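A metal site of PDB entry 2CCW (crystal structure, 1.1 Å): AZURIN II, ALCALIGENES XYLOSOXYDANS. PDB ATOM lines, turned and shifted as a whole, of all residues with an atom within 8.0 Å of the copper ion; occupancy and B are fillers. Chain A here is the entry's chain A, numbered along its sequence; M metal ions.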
ATOM      1  N   SER A   9      -4.876 -23.701 -19.196  1.00  0.00           N
ATOM      2  CA  SER A   9      -4.748 -22.632 -20.188  1.00  0.00           C
ATOM      3  C   SER A   9      -3.862 -21.550 -19.569  1.00  0.00           C
ATOM      4  O   SER A   9      -3.901 -21.360 -18.368  1.00  0.00           O
ATOM      5  CB  SER A   9      -6.130 -22.112 -20.558  1.00  0.00           C
ATOM      6  OG  SER A   9      -6.838 -21.566 -19.436  1.00  0.00           O
ATOM      7  N   ASN A  10      -3.102 -20.841 -20.408  1.00  0.00           N
ATOM      8  CA  ASN A  10      -2.079 -19.956 -19.894  1.00  0.00           C
ATOM      9  C   ASN A  10      -2.031 -18.624 -20.601  1.00  0.00           C
ATOM     10  O   ASN A  10      -2.857 -18.311 -21.446  1.00  0.00           O
ATOM     11  CB  ASN A  10      -0.731 -20.696 -19.878  1.00  0.00           C
ATOM     12  CG  ASN A  10      -0.147 -20.894 -21.253  1.00  0.00           C
ATOM     13  OD1 ASN A  10      -0.607 -20.317 -22.231  1.00  0.00           O
ATOM     14  ND2 ASN A  10       0.906 -21.713 -21.308  1.00  0.00           N
ATOM     15  N   MET A  13      -1.637 -18.217 -24.686  1.00  0.00           N
ATOM     16  CA  MET A  13      -2.680 -18.660 -25.600  1.00  0.00           C
ATOM     17  C   MET A  13      -2.459 -20.139 -25.933  1.00  0.00           C
ATOM     18  O   MET A  13      -2.560 -20.573 -27.068  1.00  0.00           O
ATOM     19  CB  MET A  13      -2.878 -17.717 -26.813  1.00  0.00           C
ATOM     20  CG  MET A  13      -4.303 -17.313 -27.254  1.00  0.00           C
ATOM     21  SD  MET A  13      -4.278 -16.240 -28.740  1.00  0.00           S
ATOM     22  CE  MET A  13      -4.228 -15.052 -27.160  1.00  0.00           C
ATOM     23  N   GLN A  14      -2.203 -20.936 -24.907  1.00  0.00           N
ATOM     24  CA  GLN A  14      -2.047 -22.368 -25.060  1.00  0.00           C
ATOM     25  C   GLN A  14      -2.898 -23.177 -24.099  1.00  0.00           C
ATOM     26  O   GLN A  14      -3.058 -22.787 -22.949  1.00  0.00           O
ATOM     27  CB  GLN A  14      -0.599 -22.791 -24.800  1.00  0.00           C
ATOM     28  CG  GLN A  14       0.506 -22.120 -25.535  1.00  0.00           C
ATOM     29  CD  GLN A  14       1.921 -22.498 -24.968  1.00  0.00           C
ATOM     30  OE1 GLN A  14       2.163 -22.531 -23.745  1.00  0.00           O
ATOM     31  NE2 GLN A  14       2.842 -22.785 -25.884  1.00  0.00           N
ATOM     32  N   TYR A  15      -3.416 -24.307 -24.582  1.00  0.00           N
ATOM     33  CA  TYR A  15      -3.839 -25.411 -23.738  1.00  0.00           C
ATOM     34  C   TYR A  15      -2.656 -26.370 -23.569  1.00  0.00           C
ATOM     35  O   TYR A  15      -1.867 -26.538 -24.492  1.00  0.00           O
ATOM     36  CB  TYR A  15      -4.970 -26.210 -24.425  1.00  0.00           C
ATOM     37  CG  TYR A  15      -6.350 -25.590 -24.468  1.00  0.00           C
ATOM     38  CD1 TYR A  15      -6.898 -24.804 -23.473  1.00  0.00           C
ATOM     39  CD2 TYR A  15      -7.158 -25.926 -25.529  1.00  0.00           C
ATOM     40  CE1 TYR A  15      -8.207 -24.331 -23.549  1.00  0.00           C
ATOM     41  CE2 TYR A  15      -8.444 -25.486 -25.578  1.00  0.00           C
ATOM     42  CZ  TYR A  15      -8.997 -24.699 -24.612  1.00  0.00           C
ATOM     43  OH  TYR A  15     -10.314 -24.326 -24.729  1.00  0.00           O
ATOM     44  N   LEU A  33     -11.355 -26.791 -16.404  1.00  0.00           N
ATOM     45  CA  LEU A  33     -10.447 -25.804 -17.003  1.00  0.00           C
ATOM     46  C   LEU A  33      -9.830 -25.002 -15.879  1.00  0.00           C
ATOM     47  O   LEU A  33     -10.528 -24.502 -15.008  1.00  0.00           O
ATOM     48  CB  LEU A  33     -11.206 -24.883 -17.961  1.00  0.00           C
ATOM     49  CG  LEU A  33     -10.326 -23.824 -18.658  1.00  0.00           C
ATOM     50  CD1 LEU A  33      -9.378 -24.498 -19.637  1.00  0.00           C
ATOM     51  CD2 LEU A  33     -11.195 -22.829 -19.358  1.00  0.00           C
ATOM     52  N   HIS A  35      -7.079 -21.648 -15.402  1.00  0.00           N
ATOM     53  CA  HIS A  35      -6.290 -20.573 -16.040  1.00  0.00           C
ATOM     54  C   HIS A  35      -5.082 -20.345 -15.119  1.00  0.00           C
ATOM     55  O   HIS A  35      -5.256 -19.794 -14.016  1.00  0.00           O
ATOM     56  CB  HIS A  35      -7.130 -19.325 -16.211  1.00  0.00           C
ATOM     57  CG  HIS A  35      -6.460 -18.289 -17.053  1.00  0.00           C
ATOM     58  ND1 HIS A  35      -5.110 -18.037 -17.070  1.00  0.00           N
ATOM     59  CD2 HIS A  35      -7.031 -17.440 -17.937  1.00  0.00           C
ATOM     60  CE1 HIS A  35      -4.878 -17.063 -17.953  1.00  0.00           C
ATOM     61  NE2 HIS A  35      -6.037 -16.651 -18.477  1.00  0.00           N
ATOM     62  N   ALA A  43      -8.211  -9.236 -21.117  1.00  0.00           N
ATOM     63  CA  ALA A  43      -7.078  -9.374 -21.993  1.00  0.00           C
ATOM     64  C   ALA A  43      -6.899 -10.754 -22.521  1.00  0.00           C
ATOM     65  O   ALA A  43      -6.509 -10.893 -23.654  1.00  0.00           O
ATOM     66  CB  ALA A  43      -5.795  -8.953 -21.226  1.00  0.00           C
ATOM     67  N   MET A  44      -7.154 -11.743 -21.675  1.00  0.00           N
ATOM     68  CA  MET A  44      -6.785 -13.097 -21.995  1.00  0.00           C
ATOM     69  C   MET A  44      -7.594 -14.092 -21.211  1.00  0.00           C
ATOM     70  O   MET A  44      -7.096 -15.002 -20.594  1.00  0.00           O
ATOM     71  CB  MET A  44      -5.270 -13.240 -21.606  1.00  0.00           C
ATOM     72  CG  MET A  44      -4.510 -14.583 -21.621  1.00  0.00           C
ATOM     73  SD  MET A  44      -4.268 -15.029 -23.335  1.00  0.00           S
ATOM     74  CE  MET A  44      -2.938 -13.922 -23.830  1.00  0.00           C
ATOM     75  N   GLY A  45      -8.924 -13.915 -21.280  1.00  0.00           N
ATOM     76  CA  GLY A  45      -9.814 -14.904 -20.728  1.00  0.00           C
ATOM     77  C   GLY A  45      -9.782 -16.171 -21.579  1.00  0.00           C
ATOM     78  O   GLY A  45      -9.516 -16.141 -22.760  1.00  0.00           O
ATOM     79  N   HIS A  46     -10.135 -17.270 -20.927  1.00  0.00           N
ATOM     80  CA  HIS A  46     -10.234 -18.560 -21.607  1.00  0.00           C
ATOM     81  C   HIS A  46     -11.492 -19.303 -21.162  1.00  0.00           C
ATOM     82  O   HIS A  46     -11.936 -19.217 -20.059  1.00  0.00           O
ATOM     83  CB  HIS A  46      -9.035 -19.477 -21.354  1.00  0.00           C
ATOM     84  CG  HIS A  46      -7.712 -18.905 -21.744  1.00  0.00           C
ATOM     85  ND1 HIS A  46      -7.462 -18.406 -23.012  1.00  0.00           N
ATOM     86  CD2 HIS A  46      -6.557 -18.795 -21.039  1.00  0.00           C
ATOM     87  CE1 HIS A  46      -6.199 -18.034 -23.037  1.00  0.00           C
ATOM     88  NE2 HIS A  46      -5.619 -18.228 -21.877  1.00  0.00           N
ATOM     89  N   ASN A  47     -12.017 -20.080 -22.106  1.00  0.00           N
ATOM     90  CA  ASN A  47     -13.031 -21.075 -21.819  1.00  0.00           C
ATOM     91  C   ASN A  47     -12.657 -22.370 -22.518  1.00  0.00           C
ATOM     92  O   ASN A  47     -11.612 -22.484 -23.150  1.00  0.00           O
ATOM     93  CB  ASN A  47     -14.449 -20.590 -22.140  1.00  0.00           C
ATOM     94  CG  ASN A  47     -14.690 -20.340 -23.607  1.00  0.00           C
ATOM     95  OD1 ASN A  47     -13.892 -20.736 -24.441  1.00  0.00           O
ATOM     96  ND2 ASN A  47     -15.784 -19.685 -23.963  1.00  0.00           N
ATOM     97  N   LEU A  48     -13.550 -23.352 -22.375  1.00  0.00           N
ATOM     98  CA  LEU A  48     -13.515 -24.576 -23.123  1.00  0.00           C
ATOM     99  C   LEU A  48     -14.915 -24.774 -23.700  1.00  0.00           C
ATOM    100  O   LEU A  48     -15.889 -24.791 -22.938  1.00  0.00           O
ATOM    101  CB  LEU A  48     -12.923 -25.650 -22.278  1.00  0.00           C
ATOM    102  CG  LEU A  48     -12.610 -26.924 -23.022  1.00  0.00           C
ATOM    103  CD1 LEU A  48     -11.475 -27.673 -22.387  1.00  0.00           C
ATOM    104  CD2 LEU A  48     -13.899 -27.761 -23.109  1.00  0.00           C
ATOM    105  N   VAL A  86     -16.037 -18.237 -19.167  1.00  0.00           N
ATOM    106  CA  VAL A  86     -14.766 -17.579 -19.408  1.00  0.00           C
ATOM    107  C   VAL A  86     -14.168 -17.245 -18.050  1.00  0.00           C
ATOM    108  O   VAL A  86     -14.821 -16.620 -17.223  1.00  0.00           O
ATOM    109  CB  VAL A  86     -14.897 -16.332 -20.293  1.00  0.00           C
ATOM    110  CG1 VAL A  86     -13.583 -15.593 -20.365  1.00  0.00           C
ATOM    111  CG2 VAL A  86     -15.357 -16.711 -21.664  1.00  0.00           C
ATOM    112  N   ILE A  87     -12.918 -17.638 -17.861  1.00  0.00           N
ATOM    113  CA  ILE A  87     -12.166 -17.386 -16.647  1.00  0.00           C
ATOM    114  C   ILE A  87     -10.882 -16.626 -16.940  1.00  0.00           C
ATOM    115  O   ILE A  87     -10.349 -16.644 -18.040  1.00  0.00           O
ATOM    116  CB  ILE A  87     -11.849 -18.732 -15.943  1.00  0.00           C
ATOM    117  CG1 ILE A  87     -11.075 -19.687 -16.836  1.00  0.00           C
ATOM    118  CG2 ILE A  87     -13.134 -19.357 -15.464  1.00  0.00           C
ATOM    119  CD1 ILE A  87     -10.605 -20.951 -16.136  1.00  0.00           C
ATOM    120  N   PHE A 111     -12.224 -26.092 -27.747  1.00  0.00           N
ATOM    121  CA  PHE A 111     -11.472 -24.900 -28.108  1.00  0.00           C
ATOM    122  C   PHE A 111     -11.928 -23.754 -27.225  1.00  0.00           C
ATOM    123  O   PHE A 111     -12.986 -23.806 -26.592  1.00  0.00           O
ATOM    124  CB  PHE A 111     -11.658 -24.558 -29.571  1.00  0.00           C
ATOM    125  CG  PHE A 111     -13.086 -24.332 -29.973  1.00  0.00           C
ATOM    126  CD1 PHE A 111     -13.909 -25.432 -30.297  1.00  0.00           C
ATOM    127  CD2 PHE A 111     -13.650 -23.054 -29.970  1.00  0.00           C
ATOM    128  CE1 PHE A 111     -15.226 -25.264 -30.600  1.00  0.00           C
ATOM    129  CE2 PHE A 111     -14.991 -22.899 -30.296  1.00  0.00           C
ATOM    130  CZ  PHE A 111     -15.752 -24.005 -30.604  1.00  0.00           C
ATOM    131  N   CYS A 112     -11.136 -22.686 -27.260  1.00  0.00           N
ATOM    132  CA  CYS A 112     -11.470 -21.466 -26.542  1.00  0.00           C
ATOM    133  C   CYS A 112     -12.173 -20.516 -27.488  1.00  0.00           C
ATOM    134  O   CYS A 112     -11.665 -20.263 -28.598  1.00  0.00           O
ATOM    135  CB  CYS A 112     -10.224 -20.823 -25.981  1.00  0.00           C
ATOM    136  SG  CYS A 112     -10.637 -19.289 -25.105  1.00  0.00           S
ATOM    137  N   SER A 113     -13.363 -20.011 -27.131  1.00  0.00           N
ATOM    138  CA  SER A 113     -14.089 -19.068 -27.958  1.00  0.00           C
ATOM    139  C   SER A 113     -13.874 -17.613 -27.611  1.00  0.00           C
ATOM    140  O   SER A 113     -14.523 -16.745 -28.191  1.00  0.00           O
ATOM    141  CB  SER A 113     -15.596 -19.378 -27.976  1.00  0.00           C
ATOM    142  OG  SER A 113     -16.195 -19.187 -26.724  1.00  0.00           O
ATOM    143  N   PHE A 114     -12.976 -17.328 -26.691  1.00  0.00           N
ATOM    144  CA  PHE A 114     -12.602 -15.933 -26.454  1.00  0.00           C
ATOM    145  C   PHE A 114     -12.080 -15.371 -27.759  1.00  0.00           C
ATOM    146  O   PHE A 114     -11.338 -16.074 -28.475  1.00  0.00           O
ATOM    147  CB  PHE A 114     -11.559 -15.844 -25.360  1.00  0.00           C
ATOM    148  CG  PHE A 114     -11.250 -14.439 -24.917  1.00  0.00           C
ATOM    149  CD1 PHE A 114     -10.342 -13.661 -25.581  1.00  0.00           C
ATOM    150  CD2 PHE A 114     -11.872 -13.918 -23.781  1.00  0.00           C
ATOM    151  CE1 PHE A 114     -10.037 -12.389 -25.161  1.00  0.00           C
ATOM    152  CE2 PHE A 114     -11.563 -12.632 -23.348  1.00  0.00           C
ATOM    153  CZ  PHE A 114     -10.644 -11.868 -24.045  1.00  0.00           C
ATOM    154  N   PRO A 115     -12.413 -14.128 -28.139  1.00  0.00           N
ATOM    155  CA  PRO A 115     -12.043 -13.636 -29.470  1.00  0.00           C
ATOM    156  C   PRO A 115     -10.582 -13.888 -29.842  1.00  0.00           C
ATOM    157  O   PRO A 115      -9.679 -13.527 -29.123  1.00  0.00           O
ATOM    158  CB  PRO A 115     -12.406 -12.145 -29.386  1.00  0.00           C
ATOM    159  CG  PRO A 115     -13.576 -12.138 -28.464  1.00  0.00           C
ATOM    160  CD  PRO A 115     -13.264 -13.168 -27.436  1.00  0.00           C
ATOM    161  N   GLY A 116     -10.428 -14.490 -31.035  1.00  0.00           N
ATOM    162  CA  GLY A 116      -9.119 -14.770 -31.581  1.00  0.00           C
ATOM    163  C   GLY A 116      -8.440 -16.027 -31.092  1.00  0.00           C
ATOM    164  O   GLY A 116      -7.481 -16.478 -31.713  1.00  0.00           O
ATOM    165  N   HIS A 117      -8.893 -16.649 -30.030  1.00  0.00           N
ATOM    166  CA  HIS A 117      -8.142 -17.707 -29.403  1.00  0.00           C
ATOM    167  C   HIS A 117      -8.288 -19.069 -30.080  1.00  0.00           C
ATOM    168  O   HIS A 117      -7.403 -19.921 -29.909  1.00  0.00           O
ATOM    169  CB  HIS A 117      -8.533 -17.845 -27.932  1.00  0.00           C
ATOM    170  CG  HIS A 117      -8.062 -16.707 -27.098  1.00  0.00           C
ATOM    171  ND1 HIS A 117      -8.051 -16.809 -25.710  1.00  0.00           N
ATOM    172  CD2 HIS A 117      -7.619 -15.465 -27.424  1.00  0.00           C
ATOM    173  CE1 HIS A 117      -7.623 -15.644 -25.264  1.00  0.00           C
ATOM    174  NE2 HIS A 117      -7.317 -14.813 -26.259  1.00  0.00           N
ATOM    175  N   TRP A 118      -9.350 -19.306 -30.832  1.00  0.00           N
ATOM    176  CA  TRP A 118      -9.607 -20.668 -31.323  1.00  0.00           C
ATOM    177  C   TRP A 118      -8.536 -21.148 -32.278  1.00  0.00           C
ATOM    178  O   TRP A 118      -8.341 -22.354 -32.414  1.00  0.00           O
ATOM    179  CB  TRP A 118     -10.977 -20.727 -32.010  1.00  0.00           C
ATOM    180  CG  TRP A 118     -11.111 -19.919 -33.251  1.00  0.00           C
ATOM    181  CD1 TRP A 118     -11.564 -18.644 -33.312  1.00  0.00           C
ATOM    182  CD2 TRP A 118     -10.806 -20.310 -34.597  1.00  0.00           C
ATOM    183  NE1 TRP A 118     -11.564 -18.204 -34.598  1.00  0.00           N
ATOM    184  CE2 TRP A 118     -11.098 -19.209 -35.408  1.00  0.00           C
ATOM    185  CE3 TRP A 118     -10.313 -21.461 -35.189  1.00  0.00           C
ATOM    186  CZ2 TRP A 118     -10.919 -19.224 -36.796  1.00  0.00           C
ATOM    187  CZ3 TRP A 118     -10.136 -21.474 -36.562  1.00  0.00           C
ATOM    188  CH2 TRP A 118     -10.443 -20.373 -37.354  1.00  0.00           C
ATOM    189  N   MET A 120      -5.374 -20.904 -31.939  1.00  0.00           N
ATOM    190  CA  MET A 120      -4.273 -21.401 -31.127  1.00  0.00           C
ATOM    191  C   MET A 120      -4.666 -22.415 -30.073  1.00  0.00           C
ATOM    192  O   MET A 120      -3.835 -23.198 -29.658  1.00  0.00           O
ATOM    193  CB  MET A 120      -3.650 -20.197 -30.337  1.00  0.00           C
ATOM    194  CG  MET A 120      -3.213 -19.005 -31.146  1.00  0.00           C
ATOM    195  SD  MET A 120      -1.501 -19.225 -31.577  1.00  0.00           S
ATOM    196  CE  MET A 120      -0.613 -18.900 -30.039  1.00  0.00           C
ATOM    197  N   MET A 121      -5.881 -22.366 -29.613  1.00  0.00           N
ATOM    198  CA  MET A 121      -6.333 -23.133 -28.443  1.00  0.00           C
ATOM    199  C   MET A 121      -7.420 -24.091 -28.857  1.00  0.00           C
ATOM    200  O   MET A 121      -8.627 -23.781 -28.810  1.00  0.00           O
ATOM    201  CB  MET A 121      -6.807 -22.182 -27.348  1.00  0.00           C
ATOM    202  CG  MET A 121      -5.752 -21.223 -26.938  1.00  0.00           C
ATOM    203  SD  MET A 121      -6.230 -20.141 -25.592  1.00  0.00           S
ATOM    204  CE  MET A 121      -6.397 -21.286 -24.267  1.00  0.00           C
HETATM  205 CU    CU M   1      -8.736 -18.307 -24.585  1.00  0.00          CU
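A ring nitrogen (ND1) of His 117 lies close to the backbone carbonyl oxygen of Gly 45 (3.4 Å). ND1 of His 117 lies close to SD of Met 121, at 3.8 Å. The side-chain sulfur (SD) of Met 121 lies close to a ring nitrogen (ND1) of His 46 (3.3 Å). NE2 of His 46 lies close to SD of Met 44, 3.8 Å away. The backbone carbonyl oxygen of Met 121 sits at hydrogen-bond distance from the backbone NH of Cys 112, 3.1 Å away. SG of Cys 112 lies close to N of Phe 114. The side-chain sulfur (SG) of Cys 112 lies close to the backbone NH (N) of Asn 47, at 3.4 Å. The backbone carbonyl oxygen of Cys 112 sits at hydrogen-bond distance from the backbone NH of Trp 118 (3.4 Å).
Merely in contact with the copper ion: Gly 45 (2.9 Å), Phe 114 (3.8 Å) and Met 121 (3.3 Å). Of the 25 residues printed, 6 come within 4 Å of the copper ion. The nearest printed residue that does not touch the copper ion is Asn 47 (4.5 Å).
The copper ion is bound by ND1 of His 117, ND1 of His 46 and SG of Cys 112.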
